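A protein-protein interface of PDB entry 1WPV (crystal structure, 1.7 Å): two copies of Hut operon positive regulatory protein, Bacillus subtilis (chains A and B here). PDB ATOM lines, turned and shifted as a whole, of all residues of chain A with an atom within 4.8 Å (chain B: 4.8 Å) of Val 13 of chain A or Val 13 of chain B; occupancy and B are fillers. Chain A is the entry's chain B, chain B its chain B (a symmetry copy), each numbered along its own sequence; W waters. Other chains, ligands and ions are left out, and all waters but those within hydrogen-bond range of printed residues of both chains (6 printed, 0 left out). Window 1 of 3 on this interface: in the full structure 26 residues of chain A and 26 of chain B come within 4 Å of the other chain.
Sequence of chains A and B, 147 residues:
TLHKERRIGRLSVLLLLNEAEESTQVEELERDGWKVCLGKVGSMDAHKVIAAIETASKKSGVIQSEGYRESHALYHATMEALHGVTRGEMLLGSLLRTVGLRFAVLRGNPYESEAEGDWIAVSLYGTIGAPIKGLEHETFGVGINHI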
ATOM      1  N   GLY A   9       4.658   7.882 -27.679  1.00  0.00           N
ATOM      2  CA  GLY A   9       4.652   6.577 -28.317  1.00  0.00           C
ATOM      3  C   GLY A   9       5.690   5.639 -27.723  1.00  0.00           C
ATOM      4  O   GLY A   9       5.378   4.530 -27.285  1.00  0.00           O
ATOM      5  N   ARG A  10       6.938   6.087 -27.723  1.00  0.00           N
ATOM      6  CA  ARG A  10       8.047   5.310 -27.191  1.00  0.00           C
ATOM      7  C   ARG A  10       7.784   4.875 -25.748  1.00  0.00           C
ATOM      8  O   ARG A  10       7.976   3.708 -25.387  1.00  0.00           O
ATOM      9  CB  ARG A  10       9.320   6.155 -27.259  1.00  0.00           C
ATOM     10  CG  ARG A  10      10.536   5.538 -26.614  1.00  0.00           C
ATOM     11  CD  ARG A  10      11.776   6.339 -26.975  1.00  0.00           C
ATOM     12  NE  ARG A  10      12.966   5.765 -26.363  1.00  0.00           N
ATOM     13  CZ  ARG A  10      13.317   5.960 -25.098  1.00  0.00           C
ATOM     14  NH1 ARG A  10      12.578   6.724 -24.308  1.00  0.00           N
ATOM     15  NH2 ARG A  10      14.398   5.371 -24.618  1.00  0.00           N
ATOM     16  N   LEU A  11       7.336   5.823 -24.935  1.00  0.00           N
ATOM     17  CA  LEU A  11       7.052   5.570 -23.529  1.00  0.00           C
ATOM     18  C   LEU A  11       5.971   4.520 -23.327  1.00  0.00           C
ATOM     19  O   LEU A  11       6.092   3.649 -22.466  1.00  0.00           O
ATOM     20  CB  LEU A  11       6.641   6.872 -22.838  1.00  0.00           C
ATOM     21  CG  LEU A  11       7.761   7.913 -22.730  1.00  0.00           C
ATOM     22  CD1 LEU A  11       7.228   9.194 -22.101  1.00  0.00           C
ATOM     23  CD2 LEU A  11       8.896   7.335 -21.903  1.00  0.00           C
ATOM     24  N   SER A  12       4.912   4.603 -24.121  1.00  0.00           N
ATOM     25  CA  SER A  12       3.824   3.647 -23.994  1.00  0.00           C
ATOM     26  C   SER A  12       4.295   2.245 -24.364  1.00  0.00           C
ATOM     27  O   SER A  12       3.845   1.260 -23.783  1.00  0.00           O
ATOM     28  CB  SER A  12       2.649   4.061 -24.879  1.00  0.00           C
ATOM     29  OG  SER A  12       2.974   3.988 -26.257  1.00  0.00           O
ATOM     30  N   VAL A  13       5.214   2.162 -25.323  1.00  0.00           N
ATOM     31  CA  VAL A  13       5.741   0.875 -25.767  1.00  0.00           C
ATOM     32  C   VAL A  13       6.742   0.282 -24.769  1.00  0.00           C
ATOM     33  O   VAL A  13       6.753  -0.929 -24.543  1.00  0.00           O
ATOM     34  CB  VAL A  13       6.393   1.004 -27.162  1.00  0.00           C
ATOM     35  CG1 VAL A  13       7.096  -0.292 -27.535  1.00  0.00           C
ATOM     36  CG2 VAL A  13       5.313   1.328 -28.202  1.00  0.00           C
ATOM     37  N   LEU A  14       7.578   1.130 -24.173  1.00  0.00           N
ATOM     38  CA  LEU A  14       8.544   0.667 -23.180  1.00  0.00           C
ATOM     39  C   LEU A  14       7.769   0.094 -21.990  1.00  0.00           C
ATOM     40  O   LEU A  14       8.129  -0.949 -21.444  1.00  0.00           O
ATOM     41  CB  LEU A  14       9.438   1.822 -22.711  1.00  0.00           C
ATOM     42  CG  LEU A  14      10.513   2.314 -23.688  1.00  0.00           C
ATOM     43  CD2 LEU A  14      11.541   1.213 -23.910  1.00  0.00           C
ATOM     44  N   LEU A  15       6.708   0.795 -21.595  1.00  0.00           N
ATOM     45  CA  LEU A  15       5.860   0.362 -20.484  1.00  0.00           C
ATOM     46  C   LEU A  15       5.255  -0.994 -20.828  1.00  0.00           C
ATOM     47  O   LEU A  15       5.233  -1.920 -20.017  1.00  0.00           O
ATOM     48  CB  LEU A  15       4.739   1.381 -20.252  1.00  0.00           C
ATOM     49  CG  LEU A  15       3.744   1.022 -19.145  1.00  0.00           C
ATOM     50  CD1 LEU A  15       4.454   1.059 -17.799  1.00  0.00           C
ATOM     51  CD2 LEU A  15       2.569   1.986 -19.168  1.00  0.00           C
ATOM     52  N   LEU A  16       4.780  -1.095 -22.059  1.00  0.00           N
ATOM     53  CA  LEU A  16       4.160  -2.297 -22.566  1.00  0.00           C
ATOM     54  C   LEU A  16       5.109  -3.485 -22.622  1.00  0.00           C
ATOM     55  O   LEU A  16       4.741  -4.592 -22.245  1.00  0.00           O
ATOM     56  CB  LEU A  16       3.614  -2.012 -23.966  1.00  0.00           C
ATOM     57  CG  LEU A  16       2.657  -3.031 -24.578  1.00  0.00           C
ATOM     58  CD1 LEU A  16       1.411  -3.118 -23.720  1.00  0.00           C
ATOM     59  N   LEU A  17       6.335  -3.258 -23.081  1.00  0.00           N
ATOM     60  CA  LEU A  17       7.295  -4.348 -23.219  1.00  0.00           C
ATOM     61  C   LEU A  17       8.143  -4.699 -22.007  1.00  0.00           C
ATOM     62  O   LEU A  17       8.881  -5.685 -22.038  1.00  0.00           O
ATOM     63  CB  LEU A  17       8.226  -4.072 -24.402  1.00  0.00           C
ATOM     64  CG  LEU A  17       7.564  -4.027 -25.776  1.00  0.00           C
ATOM     65  CD1 LEU A  17       8.605  -3.696 -26.827  1.00  0.00           C
ATOM     66  CD2 LEU A  17       6.903  -5.367 -26.079  1.00  0.00           C
ATOM     67  N   SER A 123      -1.119   1.448 -27.434  1.00  0.00           N
ATOM     68  CA  SER A 123      -0.107   0.484 -27.839  1.00  0.00           C
ATOM     69  C   SER A 123      -0.532  -0.921 -27.484  1.00  0.00           C
ATOM     70  O   SER A 123      -1.107  -1.156 -26.421  1.00  0.00           O
ATOM     71  CB  SER A 123       1.230   0.817 -27.187  1.00  0.00           C
ATOM     72  OG  SER A 123       1.691   2.077 -27.650  1.00  0.00           O
ATOM     73  N   PHE A 140       2.484  -6.408 -32.814  1.00  0.00           N
ATOM     74  CA  PHE A 140       2.611  -5.081 -32.206  1.00  0.00           C
ATOM     75  C   PHE A 140       1.764  -4.062 -32.951  1.00  0.00           C
ATOM     76  O   PHE A 140       1.477  -4.222 -34.136  1.00  0.00           O
ATOM     77  CB  PHE A 140       4.037  -4.537 -32.321  1.00  0.00           C
ATOM     78  CG  PHE A 140       5.007  -5.050 -31.312  1.00  0.00           C
ATOM     79  CD1 PHE A 140       5.697  -6.239 -31.532  1.00  0.00           C
ATOM     80  CD2 PHE A 140       5.342  -4.266 -30.207  1.00  0.00           C
ATOM     81  CE1 PHE A 140       6.719  -6.636 -30.679  1.00  0.00           C
ATOM     82  CE2 PHE A 140       6.363  -4.655 -29.342  1.00  0.00           C
ATOM     83  CZ  PHE A 140       7.057  -5.842 -29.581  1.00  0.00           C
ATOM     84  N   VAL A 142       0.837   0.503 -32.642  1.00  0.00           N
ATOM     85  CA  VAL A 142       0.809   1.780 -31.927  1.00  0.00           C
ATOM     86  C   VAL A 142       0.008   2.811 -32.714  1.00  0.00           C
ATOM     87  O   VAL A 142       0.259   3.033 -33.902  1.00  0.00           O
ATOM     88  CB  VAL A 142       2.229   2.346 -31.681  1.00  0.00           C
ATOM     89  CG1 VAL A 142       2.136   3.722 -31.017  1.00  0.00           C
ATOM     90  CG2 VAL A 142       3.010   1.407 -30.805  1.00  0.00           C
ATOM     91  N   GLY B   9      10.411 -10.526 -31.552  1.00  0.00           N
ATOM     92  CA  GLY B   9       9.739  -9.256 -31.758  1.00  0.00           C
ATOM     93  C   GLY B   9      10.056  -8.248 -30.666  1.00  0.00           C
ATOM     94  O   GLY B   9      10.507  -7.133 -30.932  1.00  0.00           O
ATOM     95  N   ARG B  10       9.805  -8.646 -29.426  1.00  0.00           N
ATOM     96  CA  ARG B  10      10.055  -7.800 -28.268  1.00  0.00           C
ATOM     97  C   ARG B  10      11.502  -7.304 -28.239  1.00  0.00           C
ATOM     98  O   ARG B  10      11.766  -6.115 -28.033  1.00  0.00           O
ATOM     99  CB  ARG B  10       9.748  -8.596 -26.999  1.00  0.00           C
ATOM    100  CG  ARG B  10      10.091  -7.900 -25.706  1.00  0.00           C
ATOM    101  CD  ARG B  10       9.503  -8.667 -24.533  1.00  0.00           C
ATOM    102  NE  ARG B  10       9.821  -8.016 -23.270  1.00  0.00           N
ATOM    103  CZ  ARG B  10      10.988  -8.134 -22.647  1.00  0.00           C
ATOM    104  NH1 ARG B  10      11.948  -8.886 -23.163  1.00  0.00           N
ATOM    105  NH2 ARG B  10      11.200  -7.480 -21.520  1.00  0.00           N
ATOM    106  N   LEU B  11      12.429  -8.229 -28.455  1.00  0.00           N
ATOM    107  CA  LEU B  11      13.852  -7.917 -28.445  1.00  0.00           C
ATOM    108  C   LEU B  11      14.240  -6.903 -29.509  1.00  0.00           C
ATOM    109  O   LEU B  11      15.019  -5.986 -29.251  1.00  0.00           O
ATOM    110  CB  LEU B  11      14.668  -9.199 -28.634  1.00  0.00           C
ATOM    111  CG  LEU B  11      14.573 -10.188 -27.466  1.00  0.00           C
ATOM    112  CD1 LEU B  11      15.353 -11.456 -27.789  1.00  0.00           C
ATOM    113  CD2 LEU B  11      15.112  -9.524 -26.211  1.00  0.00           C
ATOM    114  N   SER B  12      13.698  -7.067 -30.708  1.00  0.00           N
ATOM    115  CA  SER B  12      14.017  -6.150 -31.789  1.00  0.00           C
ATOM    116  C   SER B  12      13.499  -4.751 -31.479  1.00  0.00           C
ATOM    117  O   SER B  12      14.123  -3.757 -31.843  1.00  0.00           O
ATOM    118  CB  SER B  12      13.424  -6.654 -33.104  1.00  0.00           C
ATOM    119  OG  SER B  12      12.006  -6.637 -33.084  1.00  0.00           O
ATOM    120  N   VAL B  13      12.362  -4.678 -30.790  1.00  0.00           N
ATOM    121  CA  VAL B  13      11.764  -3.395 -30.435  1.00  0.00           C
ATOM    122  C   VAL B  13      12.498  -2.714 -29.274  1.00  0.00           C
ATOM    123  O   VAL B  13      12.668  -1.494 -29.276  1.00  0.00           O
ATOM    124  CB  VAL B  13      10.267  -3.567 -30.090  1.00  0.00           C
ATOM    125  CG1 VAL B  13       9.700  -2.264 -29.548  1.00  0.00           C
ATOM    126  CG2 VAL B  13       9.499  -3.985 -31.350  1.00  0.00           C
ATOM    127  N   LEU B  14      12.933  -3.497 -28.290  1.00  0.00           N
ATOM    128  CA  LEU B  14      13.676  -2.947 -27.159  1.00  0.00           C
ATOM    129  C   LEU B  14      14.980  -2.347 -27.689  1.00  0.00           C
ATOM    130  O   LEU B  14      15.395  -1.265 -27.274  1.00  0.00           O
ATOM    131  CB  LEU B  14      13.987  -4.041 -26.129  1.00  0.00           C
ATOM    132  CG  LEU B  14      12.821  -4.537 -25.264  1.00  0.00           C
ATOM    133  CD2 LEU B  14      12.340  -3.409 -24.363  1.00  0.00           C
ATOM    134  N   LEU B  15      15.623  -3.069 -28.605  1.00  0.00           N
ATOM    135  CA  LEU B  15      16.872  -2.616 -29.217  1.00  0.00           C
ATOM    136  C   LEU B  15      16.613  -1.304 -29.949  1.00  0.00           C
ATOM    137  O   LEU B  15      17.371  -0.340 -29.843  1.00  0.00           O
ATOM    138  CB  LEU B  15      17.381  -3.667 -30.211  1.00  0.00           C
ATOM    139  CG  LEU B  15      18.661  -3.293 -30.963  1.00  0.00           C
ATOM    140  CD1 LEU B  15      19.823  -3.234 -29.982  1.00  0.00           C
ATOM    141  CD2 LEU B  15      18.930  -4.303 -32.067  1.00  0.00           C
ATOM    142  N   LEU B  16      15.510  -1.284 -30.679  1.00  0.00           N
ATOM    143  CA  LEU B  16      15.100  -0.134 -31.452  1.00  0.00           C
ATOM    144  C   LEU B  16      14.795   1.087 -30.597  1.00  0.00           C
ATOM    145  O   LEU B  16      15.197   2.195 -30.931  1.00  0.00           O
ATOM    146  CB  LEU B  16      13.863  -0.510 -32.270  1.00  0.00           C
ATOM    147  CG  LEU B  16      13.432   0.438 -33.385  1.00  0.00           C
ATOM    148  CD1 LEU B  16      14.534   0.518 -34.422  1.00  0.00           C
ATOM    149  N   LEU B  17      14.091   0.887 -29.488  1.00  0.00           N
ATOM    150  CA  LEU B  17      13.706   2.006 -28.635  1.00  0.00           C
ATOM    151  C   LEU B  17      14.692   2.450 -27.566  1.00  0.00           C
ATOM    152  O   LEU B  17      14.464   3.462 -26.902  1.00  0.00           O
ATOM    153  CB  LEU B  17      12.363   1.709 -27.965  1.00  0.00           C
ATOM    154  CG  LEU B  17      11.166   1.569 -28.902  1.00  0.00           C
ATOM    155  CD1 LEU B  17       9.930   1.228 -28.094  1.00  0.00           C
ATOM    156  CD2 LEU B  17      10.960   2.864 -29.678  1.00  0.00           C
ATOM    157  N   SER B 123      11.638  -4.325 -37.455  1.00  0.00           N
ATOM    158  CA  SER B 123      10.986  -3.342 -36.602  1.00  0.00           C
ATOM    159  C   SER B 123      11.367  -1.939 -37.012  1.00  0.00           C
ATOM    160  O   SER B 123      12.520  -1.675 -37.357  1.00  0.00           O
ATOM    161  CB  SER B 123      11.348  -3.588 -35.142  1.00  0.00           C
ATOM    162  OG  SER B 123      10.847  -4.850 -34.729  1.00  0.00           O
ATOM    163  N   PHE B 140       5.298   3.392 -35.478  1.00  0.00           N
ATOM    164  CA  PHE B 140       5.917   2.104 -35.159  1.00  0.00           C
ATOM    165  C   PHE B 140       5.413   1.016 -36.094  1.00  0.00           C
ATOM    166  O   PHE B 140       4.312   1.104 -36.634  1.00  0.00           O
ATOM    167  CB  PHE B 140       5.519   1.611 -33.765  1.00  0.00           C
ATOM    168  CG  PHE B 140       6.275   2.213 -32.629  1.00  0.00           C
ATOM    169  CD1 PHE B 140       5.864   3.415 -32.062  1.00  0.00           C
ATOM    170  CD2 PHE B 140       7.312   1.499 -32.027  1.00  0.00           C
ATOM    171  CE1 PHE B 140       6.460   3.896 -30.902  1.00  0.00           C
ATOM    172  CE2 PHE B 140       7.921   1.971 -30.866  1.00  0.00           C
ATOM    173  CZ  PHE B 140       7.490   3.171 -30.299  1.00  0.00           C
ATOM    174  N   VAL B 142       6.097  -3.562 -36.705  1.00  0.00           N
ATOM    175  CA  VAL B 142       6.852  -4.801 -36.517  1.00  0.00           C
ATOM    176  C   VAL B 142       6.297  -5.902 -37.415  1.00  0.00           C
ATOM    177  O   VAL B 142       5.093  -6.173 -37.412  1.00  0.00           O
ATOM    178  CB  VAL B 142       6.809  -5.298 -35.051  1.00  0.00           C
ATOM    179  CG1 VAL B 142       7.532  -6.642 -34.931  1.00  0.00           C
ATOM    180  CG2 VAL B 142       7.458  -4.286 -34.148  1.00  0.00           C
HETATM  181  O   HOH W   1       7.789  -8.269 -20.432  1.00  0.00           O
HETATM  182  O   HOH W   2       2.864  -6.685 -35.799  1.00  0.00           O
HETATM  183  O   HOH W   3      16.163   6.077 -27.753  1.00  0.00           O
HETATM  184  O   HOH W   4       3.349  -3.164 -35.935  1.00  0.00           O
HETATM  185  O   HOH W   5       2.293   3.536 -35.759  1.00  0.00           O
HETATM  186  O   HOH W   6       2.197   0.034 -35.140  1.00  0.00           O
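Arg 10 of chain A touches Phe 140 of chain B, and with the chains exchanged Phe 140 of chain A touches Arg 10 of chain B.
Val 13 of chain A touches its own counterpart, Val 13 of chain B.
Val 13 of chain A touches Phe 140 of chain B, and with the chains exchanged Phe 140 of chain A touches Val 13 of chain B.
Phe 140 of chain A touches Val 142 of chain B, and with the chains exchanged Val 142 of chain A touches Phe 140 of chain B.
Of the 13 pairs that touch across the chains among the printed residues, 13 have their exchanged pair printed and touching as well.
Water W5 lies within hydrogen-bond range of the backbone carbonyl oxygen (O) of Val 142 of chain A (2.8 Å) and the backbone NH (N) of Phe 140 of chain B (3.0 Å).
Water W2 bridges O of Val 142 of chain B (2.8 Å) and N of Phe 140 of chain A (3.0 Å).
Water W6 bridges O of Phe 140 of chain B and N of Val 142 of chain A.
Water W4 bridges O of Phe 140 of chain A (2.8 Å) and N of Val 142 of chain B (2.9 Å).
Water W1 bridges the backbone carbonyl oxygen (O) of Leu 17 of chain A and the guanidinium group (NE) of Arg 10 of chain B.
O of Leu 17 of chain A is in hydrogen-bond range of NE of Arg 10 of chain B (2.8 Å).
The guanidinium group (NE) of Arg 10 of chain A is in hydrogen-bond range of the backbone carbonyl oxygen (O) of Leu 17 of chain B, at 2.8 Å.
Among the printed residues, pairs that only touch across the chains: Gly 9 of chain A with Phe 140 of chain B, Arg 10 of chain A with Phe 140 of chain B, Val 13 of chain A with Val 13 of chain B, Val 13 of chain A with Leu 17 of chain B, Val 13 of chain A with Phe 140 of chain B, Leu 17 of chain A with Val 13 of chain B, Phe 140 of chain A with Gly 9 of chain B, Phe 140 of chain A with Arg 10 of chain B, Phe 140 of chain A with Val 13 of chain B, Phe 140 of chain A with Val 142 of chain B and Val 142 of chain A with Phe 140 of chain B.
Of the printed residues of chain B, Gly 9 of chain A touches Phe 140 (3.7 Å).
Val 13 of chain A touches just these residues of chain B: Val 13 (3.8 Å), Leu 17 (3.3 Å) and Phe 140 (3.5 Å).
Printed residues of chain B within 4 Å of Phe 140 of chain A: Gly 9, Arg 10, Val 13 and Val 142.
Printed residues of chain B within 4 Å of Val 142 of chain A: Phe 140 (3.7 Å).
Of chain A, only Val 13, Leu 17 and Phe 140 come within 4 Å of Val 13 of chain B.
Of the printed residues of chain A, Leu 17 of chain B touches Arg 10 and Val 13.
Printed residues of chain A within 4 Å of Phe 140 of chain B: Gly 9 (3.7 Å), Arg 10 (3.8 Å), Val 13 (3.5 Å) and Val 142 (3.7 Å).
The nearest printed residue of chain A that does not touch Val 13 of chain B is Leu 14 of chain A (6.1 Å).
Hydrophobic or aromatic side chains of chain B within 4 Å of the printed part of chain A: Val 13, Leu 17, Phe 140 and Val 142.
Along chain B the printed residues that touch a printed residue of chain A span positions 9 to 142.
Hydrophobic or aromatic side chains of chain A within 4 Å of the printed part of chain B: Val 13, Leu 17, Phe 140 and Val 142.
Among the printed residues, no Asp or Glu carboxylate lies within 4 Å of a Lys or Arg side-chain nitrogen of the other chain.
OG of Ser 12 of chain B lies within hydrogen-bond range of O of Gly 9 of chain B (2.7 Å).
O of Gly 9 of chain A sits at hydrogen-bond distance from OG of Ser 12 of chain A (2.7 Å).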
